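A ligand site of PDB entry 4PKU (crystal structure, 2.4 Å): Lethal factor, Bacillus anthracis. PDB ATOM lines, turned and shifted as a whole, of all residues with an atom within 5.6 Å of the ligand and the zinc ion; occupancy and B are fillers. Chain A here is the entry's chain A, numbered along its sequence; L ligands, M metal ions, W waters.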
ATOM      1  N   ASP A  67       4.431   9.249 -26.453  1.00  0.00           N
ATOM      2  CA  ASP A  67       5.562   8.600 -25.792  1.00  0.00           C
ATOM      3  C   ASP A  67       6.718   9.585 -25.633  1.00  0.00           C
ATOM      4  O   ASP A  67       7.763   9.255 -25.090  1.00  0.00           O
ATOM      5  CB  ASP A  67       6.033   7.374 -26.591  1.00  0.00           C
ATOM      6  CG  ASP A  67       4.893   6.426 -26.921  1.00  0.00           C
ATOM      7  OD1 ASP A  67       3.957   6.311 -26.115  1.00  0.00           O
ATOM      8  OD2 ASP A  67       4.949   5.803 -28.004  1.00  0.00           O
ATOM      9  N   PHE A  68       6.498  10.797 -26.113  1.00  0.00           N
ATOM     10  CA  PHE A  68       7.511  11.845 -26.074  1.00  0.00           C
ATOM     11  C   PHE A  68       7.495  12.533 -24.701  1.00  0.00           C
ATOM     12  O   PHE A  68       8.521  13.022 -24.226  1.00  0.00           O
ATOM     13  CB  PHE A  68       7.278  12.853 -27.210  1.00  0.00           C
ATOM     14  CG  PHE A  68       8.462  13.746 -27.509  1.00  0.00           C
ATOM     15  CD1 PHE A  68       9.113  13.652 -28.728  1.00  0.00           C
ATOM     16  CD2 PHE A  68       8.885  14.717 -26.618  1.00  0.00           C
ATOM     17  CE1 PHE A  68      10.191  14.470 -29.023  1.00  0.00           C
ATOM     18  CE2 PHE A  68       9.957  15.538 -26.901  1.00  0.00           C
ATOM     19  CZ  PHE A  68      10.607  15.417 -28.106  1.00  0.00           C
ATOM     20  N   VAL A 392      18.023  15.310 -27.861  1.00  0.00           N
ATOM     21  CA  VAL A 392      17.205  14.158 -27.526  1.00  0.00           C
ATOM     22  C   VAL A 392      17.623  13.509 -26.208  1.00  0.00           C
ATOM     23  O   VAL A 392      18.814  13.264 -25.991  1.00  0.00           O
ATOM     24  CB  VAL A 392      17.259  13.080 -28.644  1.00  0.00           C
ATOM     25  CG1 VAL A 392      16.669  11.758 -28.162  1.00  0.00           C
ATOM     26  CG2 VAL A 392      16.550  13.586 -29.891  1.00  0.00           C
ATOM     27  N   HIS A 393      16.657  13.243 -25.343  1.00  0.00           N
ATOM     28  CA  HIS A 393      16.886  12.303 -24.249  1.00  0.00           C
ATOM     29  C   HIS A 393      16.055  11.055 -24.465  1.00  0.00           C
ATOM     30  O   HIS A 393      14.866  11.128 -24.779  1.00  0.00           O
ATOM     31  CB  HIS A 393      16.557  12.909 -22.895  1.00  0.00           C
ATOM     32  CG  HIS A 393      16.722  11.940 -21.762  1.00  0.00           C
ATOM     33  ND1 HIS A 393      17.900  11.254 -21.546  1.00  0.00           N
ATOM     34  CD2 HIS A 393      15.862  11.519 -20.807  1.00  0.00           C
ATOM     35  CE1 HIS A 393      17.762  10.465 -20.504  1.00  0.00           C
ATOM     36  NE2 HIS A 393      16.532  10.606 -20.028  1.00  0.00           N
ATOM     37  N   SER A 394      16.684   9.899 -24.284  1.00  0.00           N
ATOM     38  CA  SER A 394      16.004   8.621 -24.417  1.00  0.00           C
ATOM     39  C   SER A 394      16.874   7.502 -23.870  1.00  0.00           C
ATOM     40  O   SER A 394      17.909   7.741 -23.252  1.00  0.00           O
ATOM     41  CB  SER A 394      15.664   8.351 -25.889  1.00  0.00           C
ATOM     42  OG  SER A 394      16.815   8.420 -26.703  1.00  0.00           O
ATOM     43  N   LYS A 395      16.434   6.268 -24.093  1.00  0.00           N
ATOM     44  CA  LYS A 395      17.159   5.090 -23.655  1.00  0.00           C
ATOM     45  C   LYS A 395      18.517   4.991 -24.351  1.00  0.00           C
ATOM     46  O   LYS A 395      19.551   4.829 -23.706  1.00  0.00           O
ATOM     47  CB  LYS A 395      16.353   3.823 -23.929  1.00  0.00           C
ATOM     48  CG  LYS A 395      16.990   2.557 -23.401  1.00  0.00           C
ATOM     49  CD  LYS A 395      16.859   2.494 -21.899  1.00  0.00           C
ATOM     50  CE  LYS A 395      18.015   1.729 -21.279  1.00  0.00           C
ATOM     51  NZ  LYS A 395      17.962   1.770 -19.793  1.00  0.00           N
ATOM     52  N   GLY A 396      18.485   5.119 -25.668  1.00  0.00           N
ATOM     53  CA  GLY A 396      19.686   4.987 -26.468  1.00  0.00           C
ATOM     54  C   GLY A 396      19.718   5.953 -27.638  1.00  0.00           C
ATOM     55  O   GLY A 396      18.674   6.474 -28.047  1.00  0.00           O
ATOM     56  N   LEU A 397      20.902   6.173 -28.180  1.00  0.00           N
ATOM     57  CA  LEU A 397      21.077   7.101 -29.284  1.00  0.00           C
ATOM     58  C   LEU A 397      22.324   6.747 -30.091  1.00  0.00           C
ATOM     59  O   LEU A 397      23.316   6.277 -29.526  1.00  0.00           O
ATOM     60  CB  LEU A 397      21.177   8.535 -28.761  1.00  0.00           C
ATOM     61  CG  LEU A 397      20.838   9.696 -29.695  1.00  0.00           C
ATOM     62  CD1 LEU A 397      19.424   9.556 -30.238  1.00  0.00           C
ATOM     63  CD2 LEU A 397      21.011  11.028 -28.974  1.00  0.00           C
ATOM     64  N   TYR A 398      22.270   6.949 -31.396  1.00  0.00           N
ATOM     65  CA  TYR A 398      23.474   6.878 -32.216  1.00  0.00           C
ATOM     66  C   TYR A 398      23.710   8.228 -32.885  1.00  0.00           C
ATOM     67  O   TYR A 398      22.818   8.769 -33.536  1.00  0.00           O
ATOM     68  CB  TYR A 398      23.381   5.775 -33.273  1.00  0.00           C
ATOM     69  CG  TYR A 398      24.592   5.745 -34.181  1.00  0.00           C
ATOM     70  CD1 TYR A 398      25.809   5.237 -33.736  1.00  0.00           C
ATOM     71  CD2 TYR A 398      24.532   6.245 -35.476  1.00  0.00           C
ATOM     72  CE1 TYR A 398      26.919   5.214 -34.551  1.00  0.00           C
ATOM     73  CE2 TYR A 398      25.641   6.225 -36.309  1.00  0.00           C
ATOM     74  CZ  TYR A 398      26.831   5.706 -35.835  1.00  0.00           C
ATOM     75  OH  TYR A 398      27.947   5.688 -36.655  1.00  0.00           O
ATOM     76  N   GLY A 413      13.129   2.339 -21.996  1.00  0.00           N
ATOM     77  CA  GLY A 413      12.865   2.553 -23.403  1.00  0.00           C
ATOM     78  C   GLY A 413      11.451   2.110 -23.746  1.00  0.00           C
ATOM     79  O   GLY A 413      10.914   1.199 -23.105  1.00  0.00           O
ATOM     80  N   VAL A 414      10.842   2.747 -24.738  1.00  0.00           N
ATOM     81  CA  VAL A 414       9.483   2.390 -25.104  1.00  0.00           C
ATOM     82  C   VAL A 414       9.471   1.031 -25.818  1.00  0.00           C
ATOM     83  O   VAL A 414      10.181   0.805 -26.790  1.00  0.00           O
ATOM     84  CB  VAL A 414       8.803   3.504 -25.974  1.00  0.00           C
ATOM     85  CG1 VAL A 414       9.457   3.635 -27.340  1.00  0.00           C
ATOM     86  CG2 VAL A 414       7.305   3.232 -26.107  1.00  0.00           C
ATOM     87  N   GLU A 415       8.675   0.121 -25.260  1.00  0.00           N
ATOM     88  CA  GLU A 415       8.552  -1.248 -25.761  1.00  0.00           C
ATOM     89  C   GLU A 415       9.903  -1.965 -25.913  1.00  0.00           C
ATOM     90  O   GLU A 415      10.126  -2.713 -26.858  1.00  0.00           O
ATOM     91  CB  GLU A 415       7.806  -1.252 -27.096  1.00  0.00           C
ATOM     92  CG  GLU A 415       6.346  -0.838 -26.962  1.00  0.00           C
ATOM     93  CD  GLU A 415       5.618  -0.795 -28.291  1.00  0.00           C
ATOM     94  OE1 GLU A 415       6.291  -0.899 -29.342  1.00  0.00           O
ATOM     95  OE2 GLU A 415       4.380  -0.651 -28.282  1.00  0.00           O
ATOM     96  N   LEU A 416      10.799  -1.714 -24.955  1.00  0.00           N
ATOM     97  CA  LEU A 416      12.039  -2.468 -24.822  1.00  0.00           C
ATOM     98  C   LEU A 416      11.976  -3.328 -23.571  1.00  0.00           C
ATOM     99  O   LEU A 416      11.463  -2.890 -22.540  1.00  0.00           O
ATOM    100  CB  LEU A 416      13.250  -1.536 -24.761  1.00  0.00           C
ATOM    101  CG  LEU A 416      13.889  -1.023 -26.044  1.00  0.00           C
ATOM    102  CD1 LEU A 416      15.015  -0.066 -25.707  1.00  0.00           C
ATOM    103  CD2 LEU A 416      14.398  -2.173 -26.897  1.00  0.00           C
ATOM    104  N   GLU A 421      18.749  -5.204 -25.604  1.00  0.00           N
ATOM    105  CA  GLU A 421      17.959  -5.021 -26.809  1.00  0.00           C
ATOM    106  C   GLU A 421      18.062  -3.586 -27.274  1.00  0.00           C
ATOM    107  O   GLU A 421      18.140  -3.300 -28.466  1.00  0.00           O
ATOM    108  CB  GLU A 421      16.498  -5.415 -26.588  1.00  0.00           C
ATOM    109  CG  GLU A 421      16.308  -6.863 -26.157  1.00  0.00           C
ATOM    110  CD  GLU A 421      14.848  -7.283 -26.156  1.00  0.00           C
ATOM    111  OE1 GLU A 421      13.975  -6.416 -25.917  1.00  0.00           O
ATOM    112  OE2 GLU A 421      14.580  -8.477 -26.414  1.00  0.00           O
ATOM    113  N   GLY A 422      18.073  -2.666 -26.305  1.00  0.00           N
ATOM    114  CA  GLY A 422      18.253  -1.265 -26.585  1.00  0.00           C
ATOM    115  C   GLY A 422      19.589  -0.939 -27.227  1.00  0.00           C
ATOM    116  O   GLY A 422      19.669  -0.086 -28.112  1.00  0.00           O
ATOM    117  N   HIS A 425      19.754  -2.117 -31.051  1.00  0.00           N
ATOM    118  CA  HIS A 425      19.029  -1.214 -31.928  1.00  0.00           C
ATOM    119  C   HIS A 425      19.928  -0.052 -32.370  1.00  0.00           C
ATOM    120  O   HIS A 425      19.949   0.306 -33.543  1.00  0.00           O
ATOM    121  CB  HIS A 425      17.767  -0.704 -31.238  1.00  0.00           C
ATOM    122  CG  HIS A 425      17.172   0.526 -31.849  1.00  0.00           C
ATOM    123  ND1 HIS A 425      16.072   0.487 -32.668  1.00  0.00           N
ATOM    124  CD2 HIS A 425      17.514   1.831 -31.716  1.00  0.00           C
ATOM    125  CE1 HIS A 425      15.766   1.720 -33.042  1.00  0.00           C
ATOM    126  NE2 HIS A 425      16.624   2.550 -32.481  1.00  0.00           N
ATOM    127  N   GLU A 426      20.657   0.515 -31.416  1.00  0.00           N
ATOM    128  CA  GLU A 426      21.587   1.610 -31.705  1.00  0.00           C
ATOM    129  C   GLU A 426      22.720   1.132 -32.614  1.00  0.00           C
ATOM    130  O   GLU A 426      23.191   1.874 -33.477  1.00  0.00           O
ATOM    131  CB  GLU A 426      22.176   2.182 -30.419  1.00  0.00           C
ATOM    132  CG  GLU A 426      21.196   2.889 -29.494  1.00  0.00           C
ATOM    133  CD  GLU A 426      20.192   3.770 -30.224  1.00  0.00           C
ATOM    134  OE1 GLU A 426      20.577   4.478 -31.170  1.00  0.00           O
ATOM    135  OE2 GLU A 426      19.010   3.757 -29.826  1.00  0.00           O
ATOM    136  N   HIS A 429      21.926   1.240 -36.162  1.00  0.00           N
ATOM    137  CA  HIS A 429      22.154   2.545 -36.767  1.00  0.00           C
ATOM    138  C   HIS A 429      23.587   2.656 -37.270  1.00  0.00           C
ATOM    139  O   HIS A 429      23.838   3.181 -38.357  1.00  0.00           O
ATOM    140  CB  HIS A 429      21.884   3.666 -35.770  1.00  0.00           C
ATOM    141  CG  HIS A 429      20.429   3.887 -35.508  1.00  0.00           C
ATOM    142  ND1 HIS A 429      19.496   4.007 -36.514  1.00  0.00           N
ATOM    143  CD2 HIS A 429      19.750   4.025 -34.347  1.00  0.00           C
ATOM    144  CE1 HIS A 429      18.301   4.203 -35.985  1.00  0.00           C
ATOM    145  NE2 HIS A 429      18.428   4.209 -34.674  1.00  0.00           N
ATOM    146  N   TYR A 467       7.034   1.438 -33.439  1.00  0.00           N
ATOM    147  CA  TYR A 467       8.035   2.493 -33.520  1.00  0.00           C
ATOM    148  C   TYR A 467       8.817   2.404 -34.818  1.00  0.00           C
ATOM    149  O   TYR A 467       9.311   3.415 -35.326  1.00  0.00           O
ATOM    150  CB  TYR A 467       8.994   2.408 -32.323  1.00  0.00           C
ATOM    151  CG  TYR A 467      10.075   3.463 -32.372  1.00  0.00           C
ATOM    152  CD1 TYR A 467       9.761   4.809 -32.502  1.00  0.00           C
ATOM    153  CD2 TYR A 467      11.422   3.110 -32.294  1.00  0.00           C
ATOM    154  CE1 TYR A 467      10.741   5.770 -32.556  1.00  0.00           C
ATOM    155  CE2 TYR A 467      12.410   4.073 -32.336  1.00  0.00           C
ATOM    156  CZ  TYR A 467      12.059   5.402 -32.473  1.00  0.00           C
ATOM    157  OH  TYR A 467      13.046   6.357 -32.522  1.00  0.00           O
ATOM    158  N   GLU A 474      14.715   4.154 -38.415  1.00  0.00           N
ATOM    159  CA  GLU A 474      14.133   3.447 -37.285  1.00  0.00           C
ATOM    160  C   GLU A 474      13.686   2.037 -37.657  1.00  0.00           C
ATOM    161  O   GLU A 474      13.871   1.100 -36.894  1.00  0.00           O
ATOM    162  CB  GLU A 474      12.958   4.240 -36.713  1.00  0.00           C
ATOM    163  CG  GLU A 474      13.323   5.620 -36.196  1.00  0.00           C
ATOM    164  CD  GLU A 474      14.481   5.562 -35.213  1.00  0.00           C
ATOM    165  OE1 GLU A 474      14.548   4.579 -34.459  1.00  0.00           O
ATOM    166  OE2 GLU A 474      15.300   6.506 -35.200  1.00  0.00           O
ATOM    167  N   ALA A 477      16.799  -0.159 -37.916  1.00  0.00           N
ATOM    168  CA  ALA A 477      17.363  -0.466 -36.610  1.00  0.00           C
ATOM    169  C   ALA A 477      16.481  -1.439 -35.831  1.00  0.00           C
ATOM    170  O   ALA A 477      16.971  -2.328 -35.142  1.00  0.00           O
ATOM    171  CB  ALA A 477      17.578   0.801 -35.813  1.00  0.00           C
ATOM    172  N   GLU A 478      15.162  -1.258 -35.937  1.00  0.00           N
ATOM    173  CA  GLU A 478      14.218  -2.141 -35.259  1.00  0.00           C
ATOM    174  C   GLU A 478      14.252  -3.541 -35.834  1.00  0.00           C
ATOM    175  O   GLU A 478      14.219  -4.521 -35.099  1.00  0.00           O
ATOM    176  CB  GLU A 478      12.802  -1.566 -35.342  1.00  0.00           C
ATOM    177  CG  GLU A 478      12.510  -0.464 -34.335  1.00  0.00           C
ATOM    178  CD  GLU A 478      12.554  -0.971 -32.900  1.00  0.00           C
ATOM    179  OE1 GLU A 478      11.485  -1.273 -32.346  1.00  0.00           O
ATOM    180  OE2 GLU A 478      13.662  -1.046 -32.327  1.00  0.00           O
ATOM    181  N   ARG A 481      17.473  -5.174 -34.750  1.00  0.00           N
ATOM    182  CA  ARG A 481      17.365  -5.603 -33.361  1.00  0.00           C
ATOM    183  C   ARG A 481      16.567  -6.899 -33.242  1.00  0.00           C
ATOM    184  O   ARG A 481      17.008  -7.845 -32.589  1.00  0.00           O
ATOM    185  CB  ARG A 481      16.709  -4.507 -32.505  1.00  0.00           C
ATOM    186  CG  ARG A 481      16.291  -4.994 -31.132  1.00  0.00           C
ATOM    187  CD  ARG A 481      15.671  -3.876 -30.304  1.00  0.00           C
ATOM    188  NE  ARG A 481      14.344  -3.488 -30.769  1.00  0.00           N
ATOM    189  CZ  ARG A 481      13.224  -4.123 -30.456  1.00  0.00           C
ATOM    190  NH1 ARG A 481      13.270  -5.199 -29.674  1.00  0.00           N
ATOM    191  NH2 ARG A 481      12.062  -3.701 -30.935  1.00  0.00           N
HETATM  192  C1  LIG L   1      11.529   8.702 -26.941  1.00  0.00           C
HETATM  193  C2  LIG L   1      12.450   7.898 -27.599  1.00  0.00           C
HETATM  194  C3  LIG L   1      10.171   8.585 -27.225  1.00  0.00           C
HETATM  195  C4  LIG L   1       9.743   7.668 -28.172  1.00  0.00           C
HETATM  196  C5  LIG L   1      10.671   6.868 -28.835  1.00  0.00           C
HETATM  197  C6  LIG L   1      12.028   6.968 -28.548  1.00  0.00           C
HETATM  198  C7  LIG L   1      12.995   6.093 -29.312  1.00  0.00           C
HETATM  199  N1  LIG L   1      14.312   5.929 -28.701  1.00  0.00           N
HETATM  200  C8  LIG L   1      15.419   6.671 -29.312  1.00  0.00           C
HETATM  201  C9  LIG L   1      14.985   8.058 -29.788  1.00  0.00           C
HETATM  202  C10 LIG L   1      16.047   5.971 -30.476  1.00  0.00           C
HETATM  203  N2  LIG L   1      17.366   5.771 -30.495  1.00  0.00           N
HETATM  204  O1  LIG L   1      17.930   5.445 -31.664  1.00  0.00           O
HETATM  205  O2  LIG L   1      15.315   5.492 -31.637  1.00  0.00           O
HETATM  206  S1  LIG L   1      14.544   4.993 -27.524  1.00  0.00           S
HETATM  207  O3  LIG L   1      13.413   5.058 -26.649  1.00  0.00           O
HETATM  208  O4  LIG L   1      15.730   5.386 -26.825  1.00  0.00           O
HETATM  209  C11 LIG L   1      14.730   3.498 -28.050  1.00  0.00           C
HETATM  210  C12 LIG L   1      16.005   2.945 -28.116  1.00  0.00           C
HETATM  211  C13 LIG L   1      16.188   1.652 -28.575  1.00  0.00           C
HETATM  212  C14 LIG L   1      15.088   0.893 -28.977  1.00  0.00           C
HETATM  213  F1  LIG L   1      15.254  -0.365 -29.413  1.00  0.00           F
HETATM  214  C15 LIG L   1      13.820   1.441 -28.906  1.00  0.00           C
HETATM  215  C16 LIG L   1      13.644   2.738 -28.452  1.00  0.00           C
HETATM  216  C17 LIG L   1      12.629   0.628 -29.342  1.00  0.00           C
HETATM  217  N3  LIG L   1      11.982   9.697 -25.919  1.00  0.00           N
HETATM  218 ZN    ZN M   1      16.596   4.928 -33.172  1.00  0.00          ZN
HETATM  219  O   HOH W   1      19.582   7.214 -32.631  1.00  0.00           O
HETATM  220  O   HOH W   2      17.325   7.550 -33.590  1.00  0.00           O
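OE2 of Glu 478 lies close to F1 of the ligand (3.4 Å). Asp 67 touches the ligand. O of Val 414 touches C17 of the ligand, at 3.5 Å. CD2 of Leu 416 touches F1 of the ligand, at 3.2 Å. O of Gly 422 touches C13 of the ligand, at 3.9 Å. Arg 481 touches the ligand (NE to F1, 3.5 Å). Hydrophobic or aromatic side chains that line the ligand: Val 414, Leu 416, His 425, His 429 and Tyr 467. Along chain A the residues within 4 Å of the ligand span positions 67 to 481. The nearest printed residue that does not touch the ligand is Leu 397 (4.1 Å).
Water W1 lies within hydrogen-bond range of N of Tyr 398, OE1 of Glu 426 and N2 of the ligand.
Residues that only touch the zinc ion: Tyr 467. Of the 23 residues printed, 4 come within 4 Å of the zinc ion. The nearest printed residue that does not touch the zinc ion is Glu 426 (4.3 Å).
N2 of the ligand lies within hydrogen-bond range of OE2 of Glu 426 (2.7 Å). The backbone carbonyl oxygen (O) of His 393 sits at hydrogen-bond distance from a nitrogen (N3) of the ligand, 3.4 Å away. The backbone NH (N) of Gly 396 is in hydrogen-bond range of an oxygen (O4) of the ligand (3.0 Å). OG of Ser 394 sits close to O4 of the ligand, at 3.2 Å. N2 of the ligand lies within hydrogen-bond range of O of Gly 396 (2.9 Å). An oxygen (O2) of the ligand sits close to the side-chain hydroxyl (OH) of Tyr 467 (2.6 Å). O4 of the ligand lies within hydrogen-bond range of N of Lys 395.
The zinc ion is bound by O2 of the ligand (2.1 Å). An oxygen (O1) of the ligand binds the zinc ion (2.1 Å). OE1 of Glu 474 binds the zinc ion, 2.4 Å away. A ring nitrogen (NE2) of His 429 is bound to the zinc ion (2.5 Å). NE2 of His 425 binds the zinc ion, at 2.5 Å. The zinc ion has five donor atoms within binding distance. Slightly farther from the zinc ion lies water W2 (2.8 Å).
The side-chain carboxylate of Glu 426 lies close to the backbone NH of Leu 397 (3.5 Å). OE1 of Glu 474 sits close to OH of Tyr 467, at 3.0 Å. The side-chain carboxylate (OE1) of Glu 478 is in salt-bridge range of the guanidinium group (NH2) of Arg 481 (2.9 Å). The side-chain hydroxyl of Ser 394 is in hydrogen-bond range of the backbone carbonyl oxygen of Gly 396 (3.0 Å). The side-chain carboxylate of Glu 478 is in hydrogen-bond range of a ring nitrogen (ND1) of His 425. The side-chain carboxylate of Glu 426 is in hydrogen-bond range of the backbone NH of Tyr 398, at 3.0 Å.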
